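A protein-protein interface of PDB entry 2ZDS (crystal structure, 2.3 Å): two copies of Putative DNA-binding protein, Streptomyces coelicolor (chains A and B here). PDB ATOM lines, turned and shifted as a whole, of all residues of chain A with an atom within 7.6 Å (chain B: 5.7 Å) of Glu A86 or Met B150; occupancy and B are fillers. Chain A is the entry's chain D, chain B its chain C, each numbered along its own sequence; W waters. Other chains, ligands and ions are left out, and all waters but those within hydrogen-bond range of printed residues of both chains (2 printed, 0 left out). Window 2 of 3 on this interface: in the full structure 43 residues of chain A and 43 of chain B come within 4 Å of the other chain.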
ATOM      1  N   ILE A  83     -14.309  12.667   2.287  1.00  0.00           N
ATOM      2  CA  ILE A  83     -14.631  11.277   2.030  1.00  0.00           C
ATOM      3  C   ILE A  83     -15.039  10.634   3.344  1.00  0.00           C
ATOM      4  O   ILE A  83     -14.182  10.328   4.185  1.00  0.00           O
ATOM      5  CB  ILE A  83     -13.434  10.554   1.307  1.00  0.00           C
ATOM      6  CG1 ILE A  83     -13.054  11.350   0.045  1.00  0.00           C
ATOM      7  CG2 ILE A  83     -13.782   9.095   0.955  1.00  0.00           C
ATOM      8  CD1 ILE A  83     -11.594  11.437  -0.144  1.00  0.00           C
ATOM      9  N   ILE A  84     -16.351  10.514   3.550  1.00  0.00           N
ATOM     10  CA  ILE A  84     -16.904   9.863   4.736  1.00  0.00           C
ATOM     11  C   ILE A  84     -17.322   8.418   4.399  1.00  0.00           C
ATOM     12  O   ILE A  84     -18.113   8.161   3.473  1.00  0.00           O
ATOM     13  CB  ILE A  84     -18.131  10.638   5.312  1.00  0.00           C
ATOM     14  CG1 ILE A  84     -17.808  12.133   5.562  1.00  0.00           C
ATOM     15  CG2 ILE A  84     -18.755   9.865   6.510  1.00  0.00           C
ATOM     16  CD1 ILE A  84     -16.876  12.400   6.710  1.00  0.00           C
ATOM     17  N   ASP A  85     -16.783   7.464   5.137  1.00  0.00           N
ATOM     18  CA  ASP A  85     -16.927   6.090   4.706  1.00  0.00           C
ATOM     19  C   ASP A  85     -16.819   5.146   5.912  1.00  0.00           C
ATOM     20  O   ASP A  85     -17.013   5.600   7.040  1.00  0.00           O
ATOM     21  CB  ASP A  85     -15.958   5.779   3.502  1.00  0.00           C
ATOM     22  CG  ASP A  85     -14.454   5.837   3.860  1.00  0.00           C
ATOM     23  OD1 ASP A  85     -14.063   5.587   5.008  1.00  0.00           O
ATOM     24  OD2 ASP A  85     -13.623   6.091   2.956  1.00  0.00           O
ATOM     25  N   GLU A  86     -16.523   3.868   5.685  1.00  0.00           N
ATOM     26  CA  GLU A  86     -16.532   2.828   6.742  1.00  0.00           C
ATOM     27  C   GLU A  86     -15.498   3.079   7.836  1.00  0.00           C
ATOM     28  O   GLU A  86     -15.661   2.651   8.984  1.00  0.00           O
ATOM     29  CB  GLU A  86     -16.290   1.425   6.135  1.00  0.00           C
ATOM     30  CG  GLU A  86     -17.039   1.219   4.780  1.00  0.00           C
ATOM     31  CD  GLU A  86     -16.320   1.921   3.587  1.00  0.00           C
ATOM     32  OE1 GLU A  86     -15.112   1.637   3.358  1.00  0.00           O
ATOM     33  OE2 GLU A  86     -16.945   2.760   2.905  1.00  0.00           O
ATOM     34  N   ARG A  87     -14.422   3.765   7.466  1.00  0.00           N
ATOM     35  CA  ARG A  87     -13.392   4.140   8.414  1.00  0.00           C
ATOM     36  C   ARG A  87     -13.959   5.087   9.461  1.00  0.00           C
ATOM     37  O   ARG A  87     -13.679   4.935  10.623  1.00  0.00           O
ATOM     38  CB  ARG A  87     -12.227   4.817   7.676  1.00  0.00           C
ATOM     39  CG  ARG A  87     -11.538   3.971   6.632  1.00  0.00           C
ATOM     40  CD  ARG A  87     -10.532   4.867   5.894  1.00  0.00           C
ATOM     41  NE  ARG A  87     -11.223   5.851   5.049  1.00  0.00           N
ATOM     42  CZ  ARG A  87     -10.708   7.014   4.645  1.00  0.00           C
ATOM     43  NH1 ARG A  87      -9.484   7.346   4.958  1.00  0.00           N
ATOM     44  NH2 ARG A  87     -11.413   7.820   3.864  1.00  0.00           N
ATOM     45  N   HIS A  88     -14.740   6.075   9.029  1.00  0.00           N
ATOM     46  CA  HIS A  88     -15.462   6.953   9.945  1.00  0.00           C
ATOM     47  C   HIS A  88     -16.604   6.225  10.710  1.00  0.00           C
ATOM     48  O   HIS A  88     -16.824   6.458  11.875  1.00  0.00           O
ATOM     49  CB  HIS A  88     -16.021   8.122   9.170  1.00  0.00           C
ATOM     50  CG  HIS A  88     -14.969   8.907   8.468  1.00  0.00           C
ATOM     51  ND1 HIS A  88     -14.471   8.545   7.236  1.00  0.00           N
ATOM     52  CD2 HIS A  88     -14.320  10.042   8.829  1.00  0.00           C
ATOM     53  CE1 HIS A  88     -13.558   9.428   6.865  1.00  0.00           C
ATOM     54  NE2 HIS A  88     -13.442  10.344   7.818  1.00  0.00           N
ATOM     55  N   GLU A  89     -17.307   5.333  10.033  1.00  0.00           N
ATOM     56  CA  GLU A  89     -18.261   4.478  10.689  1.00  0.00           C
ATOM     57  C   GLU A  89     -17.678   3.716  11.879  1.00  0.00           C
ATOM     58  O   GLU A  89     -18.334   3.619  12.917  1.00  0.00           O
ATOM     59  CB  GLU A  89     -18.901   3.503   9.681  1.00  0.00           C
ATOM     60  CG  GLU A  89     -20.016   2.722  10.342  1.00  0.00           C
ATOM     61  CD  GLU A  89     -20.786   1.893   9.356  1.00  0.00           C
ATOM     62  OE1 GLU A  89     -20.295   1.704   8.208  1.00  0.00           O
ATOM     63  OE2 GLU A  89     -21.872   1.408   9.751  1.00  0.00           O
ATOM     64  N   ALA A  90     -16.463   3.181  11.721  1.00  0.00           N
ATOM     65  CA  ALA A  90     -15.759   2.403  12.783  1.00  0.00           C
ATOM     66  C   ALA A  90     -15.301   3.231  13.961  1.00  0.00           C
ATOM     67  O   ALA A  90     -15.042   2.703  15.025  1.00  0.00           O
ATOM     68  CB  ALA A  90     -14.542   1.646  12.186  1.00  0.00           C
ATOM     69  N   ILE A  91     -15.167   4.531  13.790  1.00  0.00           N
ATOM     70  CA  ILE A  91     -14.689   5.360  14.902  1.00  0.00           C
ATOM     71  C   ILE A  91     -15.757   6.261  15.549  1.00  0.00           C
ATOM     72  O   ILE A  91     -15.465   7.000  16.511  1.00  0.00           O
ATOM     73  CB  ILE A  91     -13.468   6.192  14.498  1.00  0.00           C
ATOM     74  CG1 ILE A  91     -13.772   7.114  13.325  1.00  0.00           C
ATOM     75  CG2 ILE A  91     -12.273   5.254  14.224  1.00  0.00           C
ATOM     76  CD1 ILE A  91     -12.649   8.076  13.041  1.00  0.00           C
ATOM     77  N   LEU A  92     -16.983   6.192  15.022  1.00  0.00           N
ATOM     78  CA  LEU A  92     -18.053   7.085  15.442  1.00  0.00           C
ATOM     79  C   LEU A  92     -19.104   6.314  16.186  1.00  0.00           C
ATOM     80  O   LEU A  92     -19.350   5.133  15.850  1.00  0.00           O
ATOM     81  CB  LEU A  92     -18.715   7.816  14.252  1.00  0.00           C
ATOM     82  CG  LEU A  92     -17.881   8.871  13.548  1.00  0.00           C
ATOM     83  CD1 LEU A  92     -18.569   9.375  12.270  1.00  0.00           C
ATOM     84  CD2 LEU A  92     -17.562   9.999  14.515  1.00  0.00           C
ATOM     85  N   TRP A  97     -22.958   8.637  13.295  1.00  0.00           N
ATOM     86  CA  TRP A  97     -22.953   8.059  11.973  1.00  0.00           C
ATOM     87  C   TRP A  97     -24.361   8.217  11.307  1.00  0.00           C
ATOM     88  O   TRP A  97     -24.472   8.657  10.133  1.00  0.00           O
ATOM     89  CB  TRP A  97     -22.547   6.564  12.060  1.00  0.00           C
ATOM     90  CG  TRP A  97     -22.575   5.885  10.732  1.00  0.00           C
ATOM     91  CD1 TRP A  97     -23.456   4.920  10.306  1.00  0.00           C
ATOM     92  CD2 TRP A  97     -21.671   6.123   9.646  1.00  0.00           C
ATOM     93  NE1 TRP A  97     -23.174   4.583   9.007  1.00  0.00           N
ATOM     94  CE2 TRP A  97     -22.069   5.283   8.586  1.00  0.00           C
ATOM     95  CE3 TRP A  97     -20.567   6.984   9.464  1.00  0.00           C
ATOM     96  CZ2 TRP A  97     -21.393   5.260   7.346  1.00  0.00           C
ATOM     97  CZ3 TRP A  97     -19.900   6.969   8.238  1.00  0.00           C
ATOM     98  CH2 TRP A  97     -20.318   6.112   7.195  1.00  0.00           C
ATOM     99  N   ILE B 136      -7.193   3.099  -3.597  1.00  0.00           N
ATOM    100  CA  ILE B 136      -6.666   3.044  -2.235  1.00  0.00           C
ATOM    101  C   ILE B 136      -5.691   4.182  -1.894  1.00  0.00           C
ATOM    102  O   ILE B 136      -5.297   4.338  -0.760  1.00  0.00           O
ATOM    103  CB  ILE B 136      -6.129   1.541  -2.026  1.00  0.00           C
ATOM    104  CG1 ILE B 136      -6.831   0.867  -0.893  1.00  0.00           C
ATOM    105  CG2 ILE B 136      -4.593   1.240  -2.163  1.00  0.00           C
ATOM    106  CD1 ILE B 136      -8.004   0.327  -1.400  1.00  0.00           C
ATOM    107  N   LEU B 139      -6.133   6.673   1.136  1.00  0.00           N
ATOM    108  CA  LEU B 139      -5.983   6.006   2.432  1.00  0.00           C
ATOM    109  C   LEU B 139      -4.513   5.997   2.890  1.00  0.00           C
ATOM    110  O   LEU B 139      -4.155   5.366   3.919  1.00  0.00           O
ATOM    111  CB  LEU B 139      -6.467   4.539   2.310  1.00  0.00           C
ATOM    112  CG  LEU B 139      -7.851   4.127   1.736  1.00  0.00           C
ATOM    113  CD1 LEU B 139      -8.102   2.616   1.813  1.00  0.00           C
ATOM    114  CD2 LEU B 139      -8.975   4.841   2.495  1.00  0.00           C
ATOM    115  N   PRO B 145      -8.271   4.843  10.497  1.00  0.00           N
ATOM    116  CA  PRO B 145      -7.739   3.547  10.059  1.00  0.00           C
ATOM    117  C   PRO B 145      -8.655   2.822   9.093  1.00  0.00           C
ATOM    118  O   PRO B 145      -9.868   2.771   9.294  1.00  0.00           O
ATOM    119  CB  PRO B 145      -7.624   2.736  11.374  1.00  0.00           C
ATOM    120  CG  PRO B 145      -7.730   3.722  12.459  1.00  0.00           C
ATOM    121  CD  PRO B 145      -8.525   4.869  11.956  1.00  0.00           C
ATOM    122  N   ALA B 146      -8.066   2.243   8.066  1.00  0.00           N
ATOM    123  CA  ALA B 146      -8.736   1.320   7.160  1.00  0.00           C
ATOM    124  C   ALA B 146      -8.262  -0.109   7.475  1.00  0.00           C
ATOM    125  O   ALA B 146      -7.070  -0.333   7.737  1.00  0.00           O
ATOM    126  CB  ALA B 146      -8.353   1.666   5.726  1.00  0.00           C
ATOM    127  N   PRO B 147      -9.185  -1.088   7.478  1.00  0.00           N
ATOM    128  CA  PRO B 147      -8.682  -2.479   7.660  1.00  0.00           C
ATOM    129  C   PRO B 147      -7.814  -2.993   6.515  1.00  0.00           C
ATOM    130  O   PRO B 147      -7.900  -2.500   5.376  1.00  0.00           O
ATOM    131  CB  PRO B 147      -9.942  -3.327   7.758  1.00  0.00           C
ATOM    132  CG  PRO B 147     -11.088  -2.449   7.389  1.00  0.00           C
ATOM    133  CD  PRO B 147     -10.650  -1.000   7.410  1.00  0.00           C
ATOM    134  N   GLU B 148      -6.998  -3.993   6.827  1.00  0.00           N
ATOM    135  CA  GLU B 148      -6.154  -4.638   5.845  1.00  0.00           C
ATOM    136  C   GLU B 148      -6.939  -5.189   4.651  1.00  0.00           C
ATOM    137  O   GLU B 148      -6.479  -5.088   3.516  1.00  0.00           O
ATOM    138  CB  GLU B 148      -5.274  -5.699   6.516  1.00  0.00           C
ATOM    139  CG  GLU B 148      -4.314  -6.404   5.575  1.00  0.00           C
ATOM    140  CD  GLU B 148      -3.371  -5.439   4.795  1.00  0.00           C
ATOM    141  OE1 GLU B 148      -2.908  -4.433   5.423  1.00  0.00           O
ATOM    142  OE2 GLU B 148      -3.109  -5.722   3.571  1.00  0.00           O
ATOM    143  N   SER B 149      -8.117  -5.766   4.908  1.00  0.00           N
ATOM    144  CA  SER B 149      -8.985  -6.260   3.834  1.00  0.00           C
ATOM    145  C   SER B 149      -9.320  -5.156   2.805  1.00  0.00           C
ATOM    146  O   SER B 149      -9.455  -5.450   1.637  1.00  0.00           O
ATOM    147  CB  SER B 149     -10.282  -6.819   4.425  1.00  0.00           C
ATOM    148  OG  SER B 149     -10.919  -5.811   5.188  1.00  0.00           O
ATOM    149  N   MET B 150      -9.470  -3.907   3.279  1.00  0.00           N
ATOM    150  CA  MET B 150      -9.679  -2.715   2.472  1.00  0.00           C
ATOM    151  C   MET B 150      -8.480  -2.418   1.544  1.00  0.00           C
ATOM    152  O   MET B 150      -8.696  -2.134   0.371  1.00  0.00           O
ATOM    153  CB  MET B 150     -10.043  -1.520   3.368  1.00  0.00           C
ATOM    154  CG  MET B 150     -10.534  -0.253   2.644  1.00  0.00           C
ATOM    155  SD  MET B 150     -11.188   1.447   3.655  1.00  0.00           S
ATOM    156  CE  MET B 150     -12.452   0.677   5.045  1.00  0.00           C
ATOM    157  N   ILE B 151      -7.247  -2.510   2.066  1.00  0.00           N
ATOM    158  CA  ILE B 151      -6.007  -2.300   1.294  1.00  0.00           C
ATOM    159  C   ILE B 151      -5.854  -3.374   0.241  1.00  0.00           C
ATOM    160  O   ILE B 151      -5.520  -3.097  -0.911  1.00  0.00           O
ATOM    161  CB  ILE B 151      -4.707  -2.334   2.187  1.00  0.00           C
ATOM    162  CG1 ILE B 151      -4.820  -1.455   3.447  1.00  0.00           C
ATOM    163  CG2 ILE B 151      -3.441  -1.934   1.390  1.00  0.00           C
ATOM    164  CD1 ILE B 151      -4.874   0.008   3.152  1.00  0.00           C
ATOM    165  N   GLU B 152      -6.088  -4.622   0.651  1.00  0.00           N
ATOM    166  CA  GLU B 152      -5.993  -5.761  -0.243  1.00  0.00           C
ATOM    167  C   GLU B 152      -7.021  -5.690  -1.370  1.00  0.00           C
ATOM    168  O   GLU B 152      -6.705  -6.028  -2.520  1.00  0.00           O
ATOM    169  CB  GLU B 152      -6.127  -7.069   0.517  1.00  0.00           C
ATOM    170  CG  GLU B 152      -5.996  -8.289  -0.392  1.00  0.00           C
ATOM    171  CD  GLU B 152      -4.642  -8.342  -1.169  1.00  0.00           C
ATOM    172  OE1 GLU B 152      -3.572  -8.110  -0.515  1.00  0.00           O
ATOM    173  OE2 GLU B 152      -4.652  -8.608  -2.413  1.00  0.00           O
ATOM    174  N   ARG B 153      -8.232  -5.234  -1.041  1.00  0.00           N
ATOM    175  CA  ARG B 153      -9.260  -5.063  -2.046  1.00  0.00           C
ATOM    176  C   ARG B 153      -8.800  -4.038  -3.109  1.00  0.00           C
ATOM    177  O   ARG B 153      -9.234  -4.121  -4.264  1.00  0.00           O
ATOM    178  CB  ARG B 153     -10.595  -4.605  -1.432  1.00  0.00           C
ATOM    179  CG  ARG B 153     -11.494  -5.689  -0.771  1.00  0.00           C
ATOM    180  CD  ARG B 153     -12.827  -5.034  -0.221  1.00  0.00           C
ATOM    181  NE  ARG B 153     -12.898  -4.977   1.262  1.00  0.00           N
ATOM    182  CZ  ARG B 153     -12.919  -3.850   1.994  1.00  0.00           C
ATOM    183  NH1 ARG B 153     -12.873  -2.623   1.413  1.00  0.00           N
ATOM    184  NH2 ARG B 153     -12.979  -3.950   3.331  1.00  0.00           N
ATOM    185  N   GLY B 154      -7.948  -3.079  -2.708  1.00  0.00           N
ATOM    186  CA  GLY B 154      -7.428  -2.054  -3.636  1.00  0.00           C
ATOM    187  C   GLY B 154      -6.535  -2.637  -4.704  1.00  0.00           C
ATOM    188  O   GLY B 154      -6.651  -2.299  -5.876  1.00  0.00           O
HETATM  189  O   HOH W   1     -11.412   3.516  11.193  1.00  0.00           O
HETATM  190  O   HOH W   2     -13.774  -1.107   3.071  1.00  0.00           O
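The side-chain carboxylate (OD1) of Asp A85 lies within salt-bridge range of the guanidinium group (NE) of Arg A87, 2.9 Å away.
No position is printed for both chains. Of the 5 pairs that touch across the chains among the printed residues, none has its exchanged pair printed and touching as well.
Among the printed residues, pairs that only touch across the chains: Glu A86 with Met B150, Arg A87 with Pro B145, Arg A87 with Leu B139, Arg A87 with Met B150 and Arg A87 with Ala B146.
Water W2 lies within hydrogen-bond range of NH1 of Arg B153 (2.4 Å), OE1 of Glu A86 (3.1 Å) and SD of Met B150 (3.7 Å). Water W1 bridges O of Pro B145 and O of Arg A87.
Of chain B, only Met B150 comes within 4 Å of Glu A86. Printed residues of chain B within 4 Å of Arg A87: Leu B139 (3.5 Å), Pro B145 (3.4 Å), Ala B146 (3.9 Å) and Met B150 (3.8 Å). Of the printed residues of chain A, Leu B139 touches Arg A87 (3.5 Å). Of the printed residues of chain A, Pro B145 touches Arg A87 (3.4 Å). Printed residues of chain A within 4 Å of Ala B146: Arg A87 (3.9 Å). No residue of chain A comes within 4 Å of Ser B149. Of the printed residues of chain A, Met B150 touches Glu A86 and Arg A87. Gly B154 touches none of the printed residues of chain A. The nearest residue of chain A that does not touch Met B150 is Asp A85 (5.2 Å).
Of the 12 printed residues of chain B, 4 touch a printed residue of chain A. Hydrophobic or aromatic side chains of chain B that line the printed part of chain A: Leu B139, Ala B146 and Met B150. Among the printed residues, no Asp or Glu carboxylate lies within 4 Å of a Lys or Arg side-chain nitrogen of the other chain.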
